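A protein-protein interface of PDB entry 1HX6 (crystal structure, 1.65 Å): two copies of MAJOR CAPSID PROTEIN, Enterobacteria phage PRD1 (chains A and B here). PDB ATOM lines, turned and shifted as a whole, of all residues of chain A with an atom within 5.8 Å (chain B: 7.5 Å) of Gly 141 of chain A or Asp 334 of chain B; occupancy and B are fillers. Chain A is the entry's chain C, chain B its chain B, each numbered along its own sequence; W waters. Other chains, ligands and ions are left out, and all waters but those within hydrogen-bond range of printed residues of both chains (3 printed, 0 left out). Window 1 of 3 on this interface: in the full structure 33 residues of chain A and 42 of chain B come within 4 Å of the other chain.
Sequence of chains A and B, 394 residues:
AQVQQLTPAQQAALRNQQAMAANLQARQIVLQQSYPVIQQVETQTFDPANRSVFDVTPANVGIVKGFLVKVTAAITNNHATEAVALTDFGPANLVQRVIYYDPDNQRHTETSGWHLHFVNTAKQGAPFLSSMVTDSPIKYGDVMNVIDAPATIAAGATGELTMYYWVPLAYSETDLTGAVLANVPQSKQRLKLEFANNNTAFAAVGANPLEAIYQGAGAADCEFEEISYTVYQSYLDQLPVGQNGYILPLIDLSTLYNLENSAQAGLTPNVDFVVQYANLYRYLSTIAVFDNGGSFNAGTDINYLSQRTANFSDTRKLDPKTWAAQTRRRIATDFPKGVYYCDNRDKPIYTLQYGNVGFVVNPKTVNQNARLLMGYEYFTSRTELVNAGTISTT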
ATOM      1  N   SER A 131     -24.810  13.494  13.865  1.00  0.00           N
ATOM      2  CA  SER A 131     -24.204  12.720  14.945  1.00  0.00           C
ATOM      3  C   SER A 131     -24.248  11.254  14.496  1.00  0.00           C
ATOM      4  O   SER A 131     -25.326  10.692  14.303  1.00  0.00           O
ATOM      5  CB  SER A 131     -25.002  12.849  16.239  1.00  0.00           C
ATOM      6  OG  SER A 131     -24.513  11.925  17.220  1.00  0.00           O
ATOM      7  N   MET A 132     -23.069  10.648  14.344  1.00  0.00           N
ATOM      8  CA  MET A 132     -22.921   9.251  13.920  1.00  0.00           C
ATOM      9  C   MET A 132     -23.228   8.280  15.063  1.00  0.00           C
ATOM     10  O   MET A 132     -22.757   8.474  16.186  1.00  0.00           O
ATOM     11  CB  MET A 132     -21.490   9.043  13.415  1.00  0.00           C
ATOM     12  CG  MET A 132     -21.085   7.608  13.145  1.00  0.00           C
ATOM     13  SD  MET A 132     -19.373   7.534  12.576  1.00  0.00           S
ATOM     14  CE  MET A 132     -18.505   7.560  14.108  1.00  0.00           C
ATOM     15  N   LYS A 139     -21.754   8.141  26.972  1.00  0.00           N
ATOM     16  CA  LYS A 139     -22.907   8.785  26.367  1.00  0.00           C
ATOM     17  C   LYS A 139     -22.757   9.925  25.369  1.00  0.00           C
ATOM     18  O   LYS A 139     -23.314  11.021  25.544  1.00  0.00           O
ATOM     19  CB  LYS A 139     -23.937   9.141  27.469  1.00  0.00           C
ATOM     20  CG  LYS A 139     -24.324   7.872  28.309  1.00  0.00           C
ATOM     21  CD  LYS A 139     -25.602   8.036  29.147  1.00  0.00           C
ATOM     22  CE  LYS A 139     -25.881   6.737  29.926  1.00  0.00           C
ATOM     23  NZ  LYS A 139     -27.117   6.763  30.792  1.00  0.00           N
ATOM     24  N   TYR A 140     -21.987   9.622  24.319  1.00  0.00           N
ATOM     25  CA  TYR A 140     -21.834  10.500  23.165  1.00  0.00           C
ATOM     26  C   TYR A 140     -23.166  10.261  22.461  1.00  0.00           C
ATOM     27  O   TYR A 140     -23.897   9.318  22.793  1.00  0.00           O
ATOM     28  CB  TYR A 140     -20.779   9.986  22.183  1.00  0.00           C
ATOM     29  CG  TYR A 140     -19.388   9.974  22.724  1.00  0.00           C
ATOM     30  CD1 TYR A 140     -18.635  11.144  22.742  1.00  0.00           C
ATOM     31  CD2 TYR A 140     -18.825   8.809  23.231  1.00  0.00           C
ATOM     32  CE1 TYR A 140     -17.334  11.161  23.257  1.00  0.00           C
ATOM     33  CE2 TYR A 140     -17.516   8.810  23.751  1.00  0.00           C
ATOM     34  CZ  TYR A 140     -16.783  10.004  23.754  1.00  0.00           C
ATOM     35  OH  TYR A 140     -15.493  10.041  24.246  1.00  0.00           O
ATOM     36  N   GLY A 141     -23.466  11.079  21.459  1.00  0.00           N
ATOM     37  CA  GLY A 141     -24.693  10.864  20.720  1.00  0.00           C
ATOM     38  C   GLY A 141     -25.350  12.169  20.371  1.00  0.00           C
ATOM     39  O   GLY A 141     -24.687  13.203  20.327  1.00  0.00           O
ATOM     40  N   ASP A 142     -26.646  12.121  20.082  1.00  0.00           N
ATOM     41  CA  ASP A 142     -27.368  13.349  19.781  1.00  0.00           C
ATOM     42  C   ASP A 142     -27.698  13.957  21.140  1.00  0.00           C
ATOM     43  O   ASP A 142     -28.765  13.722  21.707  1.00  0.00           O
ATOM     44  CB  ASP A 142     -28.648  13.051  18.988  1.00  0.00           C
ATOM     45  CG  ASP A 142     -29.478  14.291  18.747  1.00  0.00           C
ATOM     46  OD1 ASP A 142     -28.958  15.400  18.966  1.00  0.00           O
ATOM     47  OD2 ASP A 142     -30.650  14.150  18.343  1.00  0.00           O
ATOM     48  N   VAL A 143     -26.756  14.731  21.658  1.00  0.00           N
ATOM     49  CA  VAL A 143     -26.896  15.366  22.959  1.00  0.00           C
ATOM     50  C   VAL A 143     -27.405  16.793  22.826  1.00  0.00           C
ATOM     51  O   VAL A 143     -28.281  17.228  23.581  1.00  0.00           O
ATOM     52  CB  VAL A 143     -25.503  15.406  23.699  1.00  0.00           C
ATOM     53  CG1 VAL A 143     -25.593  16.222  25.003  1.00  0.00           C
ATOM     54  CG2 VAL A 143     -25.023  13.990  23.976  1.00  0.00           C
ATOM     55  N   MET A 144     -26.861  17.497  21.836  1.00  0.00           N
ATOM     56  CA  MET A 144     -27.158  18.907  21.620  1.00  0.00           C
ATOM     57  C   MET A 144     -28.143  19.265  20.520  1.00  0.00           C
ATOM     58  O   MET A 144     -28.427  20.443  20.335  1.00  0.00           O
ATOM     59  CB  MET A 144     -25.844  19.657  21.379  1.00  0.00           C
ATOM     60  CG  MET A 144     -24.928  19.695  22.593  1.00  0.00           C
ATOM     61  SD  MET A 144     -25.681  20.652  23.943  1.00  0.00           S
ATOM     62  CE  MET A 144     -25.770  22.322  23.159  1.00  0.00           C
ATOM     63  N   ASN A 145     -28.648  18.264  19.803  1.00  0.00           N
ATOM     64  CA  ASN A 145     -29.623  18.477  18.732  1.00  0.00           C
ATOM     65  C   ASN A 145     -29.279  19.629  17.797  1.00  0.00           C
ATOM     66  O   ASN A 145     -30.093  20.520  17.556  1.00  0.00           O
ATOM     67  CB  ASN A 145     -31.000  18.687  19.346  1.00  0.00           C
ATOM     68  CG  ASN A 145     -31.585  17.389  19.850  1.00  0.00           C
ATOM     69  OD1 ASN A 145     -31.990  16.527  19.052  1.00  0.00           O
ATOM     70  ND2 ASN A 145     -31.599  17.217  21.162  1.00  0.00           N
ATOM     71  N   VAL A 146     -28.076  19.572  17.249  1.00  0.00           N
ATOM     72  CA  VAL A 146     -27.574  20.611  16.361  1.00  0.00           C
ATOM     73  C   VAL A 146     -28.450  20.767  15.119  1.00  0.00           C
ATOM     74  O   VAL A 146     -28.826  21.887  14.777  1.00  0.00           O
ATOM     75  CB  VAL A 146     -26.106  20.312  16.016  1.00  0.00           C
ATOM     76  CG1 VAL A 146     -25.576  21.339  15.022  1.00  0.00           C
ATOM     77  CG2 VAL A 146     -25.283  20.364  17.324  1.00  0.00           C
ATOM     78  N   THR B 121     -10.737  10.415  22.152  1.00  0.00           N
ATOM     79  CA  THR B 121     -11.823  10.583  21.183  1.00  0.00           C
ATOM     80  C   THR B 121     -11.534  11.748  20.232  1.00  0.00           C
ATOM     81  O   THR B 121     -11.634  11.615  19.005  1.00  0.00           O
ATOM     82  CB  THR B 121     -13.147  10.811  21.912  1.00  0.00           C
ATOM     83  OG1 THR B 121     -13.585   9.558  22.448  1.00  0.00           O
ATOM     84  CG2 THR B 121     -14.234  11.391  20.972  1.00  0.00           C
ATOM     85  N   PRO B 127     -15.789   8.711  18.625  1.00  0.00           N
ATOM     86  CA  PRO B 127     -15.717   8.069  19.950  1.00  0.00           C
ATOM     87  C   PRO B 127     -14.609   7.018  19.909  1.00  0.00           C
ATOM     88  O   PRO B 127     -14.594   6.115  19.052  1.00  0.00           O
ATOM     89  CB  PRO B 127     -17.123   7.490  20.123  1.00  0.00           C
ATOM     90  CG  PRO B 127     -17.979   8.589  19.459  1.00  0.00           C
ATOM     91  CD  PRO B 127     -17.184   8.840  18.171  1.00  0.00           C
ATOM     92  N   LYS B 321     -25.396  25.548  21.149  1.00  0.00           N
ATOM     93  CA  LYS B 321     -25.600  24.655  20.011  1.00  0.00           C
ATOM     94  C   LYS B 321     -24.615  24.926  18.881  1.00  0.00           C
ATOM     95  O   LYS B 321     -24.170  23.997  18.204  1.00  0.00           O
ATOM     96  CB  LYS B 321     -27.041  24.728  19.479  1.00  0.00           C
ATOM     97  CG  LYS B 321     -28.027  23.795  20.199  1.00  0.00           C
ATOM     98  CD  LYS B 321     -29.298  23.570  19.379  1.00  0.00           C
ATOM     99  CE  LYS B 321     -30.330  22.738  20.144  1.00  0.00           C
ATOM    100  NZ  LYS B 321     -31.499  22.346  19.296  1.00  0.00           N
ATOM    101  N   TRP B 323     -21.616  26.124  19.308  1.00  0.00           N
ATOM    102  CA  TRP B 323     -20.343  25.631  19.821  1.00  0.00           C
ATOM    103  C   TRP B 323     -20.329  24.112  19.563  1.00  0.00           C
ATOM    104  O   TRP B 323     -19.349  23.547  19.060  1.00  0.00           O
ATOM    105  CB  TRP B 323     -20.261  25.924  21.320  1.00  0.00           C
ATOM    106  CG  TRP B 323     -18.978  25.514  21.941  1.00  0.00           C
ATOM    107  CD1 TRP B 323     -18.602  24.248  22.315  1.00  0.00           C
ATOM    108  CD2 TRP B 323     -17.877  26.369  22.249  1.00  0.00           C
ATOM    109  NE1 TRP B 323     -17.329  24.270  22.835  1.00  0.00           N
ATOM    110  CE2 TRP B 323     -16.862  25.560  22.805  1.00  0.00           C
ATOM    111  CE3 TRP B 323     -17.646  27.746  22.102  1.00  0.00           C
ATOM    112  CZ2 TRP B 323     -15.630  26.085  23.220  1.00  0.00           C
ATOM    113  CZ3 TRP B 323     -16.423  28.267  22.510  1.00  0.00           C
ATOM    114  CH2 TRP B 323     -15.432  27.436  23.064  1.00  0.00           C
ATOM    115  N   ALA B 324     -21.438  23.459  19.890  1.00  0.00           N
ATOM    116  CA  ALA B 324     -21.557  22.013  19.690  1.00  0.00           C
ATOM    117  C   ALA B 324     -21.409  21.645  18.206  1.00  0.00           C
ATOM    118  O   ALA B 324     -20.868  20.587  17.867  1.00  0.00           O
ATOM    119  CB  ALA B 324     -22.915  21.531  20.242  1.00  0.00           C
ATOM    120  N   ALA B 325     -21.903  22.510  17.319  1.00  0.00           N
ATOM    121  CA  ALA B 325     -21.786  22.251  15.888  1.00  0.00           C
ATOM    122  C   ALA B 325     -20.313  22.165  15.493  1.00  0.00           C
ATOM    123  O   ALA B 325     -19.927  21.291  14.719  1.00  0.00           O
ATOM    124  CB  ALA B 325     -22.494  23.361  15.078  1.00  0.00           C
ATOM    125  N   THR B 327     -17.868  21.205  17.312  1.00  0.00           N
ATOM    126  CA  THR B 327     -17.370  19.938  17.833  1.00  0.00           C
ATOM    127  C   THR B 327     -17.854  18.758  16.978  1.00  0.00           C
ATOM    128  O   THR B 327     -17.106  17.794  16.770  1.00  0.00           O
ATOM    129  CB  THR B 327     -17.805  19.772  19.307  1.00  0.00           C
ATOM    130  OG1 THR B 327     -17.029  20.672  20.105  1.00  0.00           O
ATOM    131  CG2 THR B 327     -17.579  18.344  19.816  1.00  0.00           C
ATOM    132  N   ARG B 328     -19.087  18.827  16.468  1.00  0.00           N
ATOM    133  CA  ARG B 328     -19.559  17.733  15.601  1.00  0.00           C
ATOM    134  C   ARG B 328     -18.669  17.591  14.364  1.00  0.00           C
ATOM    135  O   ARG B 328     -18.568  16.502  13.784  1.00  0.00           O
ATOM    136  CB  ARG B 328     -21.011  17.964  15.161  1.00  0.00           C
ATOM    137  CG  ARG B 328     -22.007  17.702  16.281  1.00  0.00           C
ATOM    138  CD  ARG B 328     -23.406  17.447  15.709  1.00  0.00           C
ATOM    139  NE  ARG B 328     -24.378  17.190  16.776  1.00  0.00           N
ATOM    140  CZ  ARG B 328     -25.619  16.755  16.573  1.00  0.00           C
ATOM    141  NH1 ARG B 328     -26.061  16.528  15.335  1.00  0.00           N
ATOM    142  NH2 ARG B 328     -26.409  16.540  17.615  1.00  0.00           N
ATOM    143  N   ILE B 331     -15.490  15.424  15.975  1.00  0.00           N
ATOM    144  CA  ILE B 331     -15.626  14.040  16.418  1.00  0.00           C
ATOM    145  C   ILE B 331     -16.866  13.326  15.903  1.00  0.00           C
ATOM    146  O   ILE B 331     -17.186  12.227  16.373  1.00  0.00           O
ATOM    147  CB  ILE B 331     -15.586  13.914  17.982  1.00  0.00           C
ATOM    148  CG1 ILE B 331     -16.739  14.682  18.619  1.00  0.00           C
ATOM    149  CG2 ILE B 331     -14.249  14.460  18.511  1.00  0.00           C
ATOM    150  CD1 ILE B 331     -17.100  14.194  20.015  1.00  0.00           C
ATOM    151  N   ALA B 332     -17.562  13.959  14.955  1.00  0.00           N
ATOM    152  CA  ALA B 332     -18.745  13.387  14.301  1.00  0.00           C
ATOM    153  C   ALA B 332     -19.953  13.094  15.180  1.00  0.00           C
ATOM    154  O   ALA B 332     -20.836  12.324  14.784  1.00  0.00           O
ATOM    155  CB  ALA B 332     -18.338  12.102  13.538  1.00  0.00           C
ATOM    156  N   THR B 333     -20.010  13.716  16.358  1.00  0.00           N
ATOM    157  CA  THR B 333     -21.109  13.511  17.290  1.00  0.00           C
ATOM    158  C   THR B 333     -20.878  14.534  18.411  1.00  0.00           C
ATOM    159  O   THR B 333     -19.968  15.353  18.310  1.00  0.00           O
ATOM    160  CB  THR B 333     -21.080  12.060  17.843  1.00  0.00           C
ATOM    161  OG1 THR B 333     -22.249  11.823  18.632  1.00  0.00           O
ATOM    162  CG2 THR B 333     -19.828  11.820  18.706  1.00  0.00           C
ATOM    163  N   ASP B 334     -21.711  14.518  19.443  1.00  0.00           N
ATOM    164  CA  ASP B 334     -21.532  15.437  20.582  1.00  0.00           C
ATOM    165  C   ASP B 334     -20.856  14.712  21.735  1.00  0.00           C
ATOM    166  O   ASP B 334     -21.015  13.502  21.881  1.00  0.00           O
ATOM    167  CB  ASP B 334     -22.884  15.903  21.142  1.00  0.00           C
ATOM    168  CG  ASP B 334     -23.742  16.612  20.114  1.00  0.00           C
ATOM    169  OD1 ASP B 334     -23.180  17.385  19.317  1.00  0.00           O
ATOM    170  OD2 ASP B 334     -24.977  16.408  20.127  1.00  0.00           O
ATOM    171  N   PHE B 335     -20.097  15.450  22.545  1.00  0.00           N
ATOM    172  CA  PHE B 335     -19.539  14.889  23.771  1.00  0.00           C
ATOM    173  C   PHE B 335     -20.759  14.803  24.716  1.00  0.00           C
ATOM    174  O   PHE B 335     -21.804  15.404  24.444  1.00  0.00           O
ATOM    175  CB  PHE B 335     -18.490  15.834  24.373  1.00  0.00           C
ATOM    176  CG  PHE B 335     -17.119  15.644  23.808  1.00  0.00           C
ATOM    177  CD1 PHE B 335     -16.342  14.566  24.217  1.00  0.00           C
ATOM    178  CD2 PHE B 335     -16.610  16.530  22.856  1.00  0.00           C
ATOM    179  CE1 PHE B 335     -15.070  14.358  23.694  1.00  0.00           C
ATOM    180  CE2 PHE B 335     -15.349  16.340  22.321  1.00  0.00           C
ATOM    181  CZ  PHE B 335     -14.565  15.253  22.735  1.00  0.00           C
ATOM    182  N   PRO B 336     -20.651  14.053  25.834  1.00  0.00           N
ATOM    183  CA  PRO B 336     -21.771  13.919  26.775  1.00  0.00           C
ATOM    184  C   PRO B 336     -22.277  15.265  27.340  1.00  0.00           C
ATOM    185  O   PRO B 336     -21.595  16.285  27.255  1.00  0.00           O
ATOM    186  CB  PRO B 336     -21.199  13.010  27.883  1.00  0.00           C
ATOM    187  CG  PRO B 336     -20.166  12.199  27.162  1.00  0.00           C
ATOM    188  CD  PRO B 336     -19.502  13.235  26.257  1.00  0.00           C
ATOM    189  N   LYS B 337     -23.474  15.245  27.910  1.00  0.00           N
ATOM    190  CA  LYS B 337     -24.088  16.445  28.480  1.00  0.00           C
ATOM    191  C   LYS B 337     -23.148  17.235  29.374  1.00  0.00           C
ATOM    192  O   LYS B 337     -22.491  16.676  30.274  1.00  0.00           O
ATOM    193  CB  LYS B 337     -25.324  16.068  29.303  1.00  0.00           C
ATOM    194  CG  LYS B 337     -26.460  15.483  28.497  1.00  0.00           C
ATOM    195  CD  LYS B 337     -27.729  15.376  29.352  1.00  0.00           C
ATOM    196  CE  LYS B 337     -27.514  14.464  30.556  1.00  0.00           C
ATOM    197  NZ  LYS B 337     -28.699  14.477  31.466  1.00  0.00           N
ATOM    198  N   VAL B 339     -20.350  18.605  28.609  1.00  0.00           N
ATOM    199  CA  VAL B 339     -18.935  18.519  28.232  1.00  0.00           C
ATOM    200  C   VAL B 339     -18.715  19.336  26.958  1.00  0.00           C
ATOM    201  O   VAL B 339     -19.332  19.053  25.932  1.00  0.00           O
ATOM    202  CB  VAL B 339     -18.511  17.062  27.957  1.00  0.00           C
ATOM    203  CG1 VAL B 339     -17.033  17.026  27.569  1.00  0.00           C
ATOM    204  CG2 VAL B 339     -18.779  16.184  29.215  1.00  0.00           C
HETATM  205  O   HOH W   1     -21.592  12.308  11.648  1.00  0.00           O
HETATM  206  O   HOH W   2     -24.716  12.547  27.481  1.00  0.00           O
HETATM  207  O   HOH W   3     -22.306   9.029  18.723  1.00  0.00           O
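Water W3 lies within hydrogen-bond range of O of Met 132 of chain A and OG1 of Thr 333 of chain B. Water W2 bridges O of Lys 139 of chain A and N of Lys 337 of chain B. Water W1 lies within hydrogen-bond range of the backbone carbonyl oxygen of Ala 332 of chain B and the backbone NH of Met 132 of chain A.
Ser 131 of chain A touches Arg 328 of chain B (N to NH1, 3.6 Å). O of Ala 332 of chain B touches CA of Ser 131 of chain A, 3.4 Å away. Asp 142 of chain A touches Asp 334 of chain B. Val 143 of chain A touches Phe 335 of chain B (CG2 to O, 3.5 Å). Val 143 of chain A touches Lys 337 of chain B. Met 144 of chain A touches Ala 324 of chain B (CG to CB, 3.6 Å). Arg 328 of chain B touches Asn 145 of chain A (NH2 to N, 3.6 Å). Val 146 of chain A touches Lys 321 of chain B. Val 146 of chain A touches Ala 324 of chain B. Val 146 of chain A touches Ala 325 of chain B (CG1 to CB, 3.7 Å).
N of Gly 141 of chain A lies within hydrogen-bond range of OG1 of Thr 333 of chain B, 3.2 Å away. N of Val 143 of chain A is in hydrogen-bond range of OD2 of Asp 334 of chain B (2.9 Å). The side-chain hydroxyl (OH) of Tyr 140 of chain A sits at hydrogen-bond distance from the side-chain hydroxyl (OG1) of Thr 121 of chain B, at 2.7 Å. The side-chain carboxylate (OD2) of Asp 334 of chain B sits at hydrogen-bond distance from the backbone NH (N) of Met 144 of chain A (2.8 Å). O of Ala 332 of chain B sits at hydrogen-bond distance from N of Met 132 of chain A (2.8 Å). NH2 of Arg 328 of chain B lies within salt-bridge range of OD1 of Asp 142 of chain A, at 3.1 Å. The backbone NH (N) of Val 146 of chain A lies close to the guanidinium group (NH2) of Arg 328 of chain B (3.5 Å). The side-chain hydroxyl of Thr 333 of chain B is in hydrogen-bond range of the side-chain hydroxyl of Ser 131 of chain A (2.7 Å). NZ of Lys 321 of chain B lies within hydrogen-bond range of O of Asn 145 of chain A. N of Asp 334 of chain B lies close to O of Gly 141 of chain A, at 3.4 Å.
OD2 of Asp 142 of chain A lies close to OD1 of Asn 145 of chain A (2.8 Å). The side-chain carboxylate (OD1) of Asp 334 of chain B is in salt-bridge range of the guanidinium group (NE) of Arg 328 of chain B, at 2.8 Å. OG of Ser 131 of chain A lies close to O of Gly 141 of chain A.
No position is printed for both chains.
Hydrophobic or aromatic side chains of chain A that line the printed part of chain B: Met 132, Tyr 140, Val 143, Met 144 and Val 146. Along chain A the printed residues that touch a printed residue of chain B span positions 131 to 146. Hydrophobic or aromatic side chains of chain B within 4 Å of the printed part of chain A: Pro 127, Ala 324, Ala 325, Phe 335 and Pro 336. Among the printed residues, Asp or Glu carboxylates within 4 Å of a Lys or Arg side-chain nitrogen of the other chain: Asp 142 of chain A with Arg 328 of chain B (3.1 Å).
Of the printed residues of chain B, Lys 139 of chain A touches Pro 336. Gly 141 of chain A touches just these residues of chain B: Thr 333 (3.2 Å) and Asp 334 (3.2 Å). Printed residues of chain B within 4 Å of Val 143 of chain A: Asp 334 (2.9 Å), Phe 335 (3.5 Å) and Lys 337 (3.7 Å). Printed residues of chain A within 4 Å of Lys 321 of chain B: Met 144 (3.0 Å), Asn 145 (2.9 Å) and Val 146 (3.9 Å). Trp 323 of chain B touches none of the printed residues of chain A. Printed residues of chain A within 4 Å of Phe 335 of chain B: Tyr 140 and Val 143. Printed residues of chain A within 4 Å of Lys 337 of chain B: Val 143 (3.7 Å). The nearest residue of chain B that does not touch Gly 141 of chain A is Arg 328 of chain B (4.6 Å). The nearest printed residue of chain A that does not touch Asp 334 of chain B is Asn 145 of chain A (4.1 Å).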
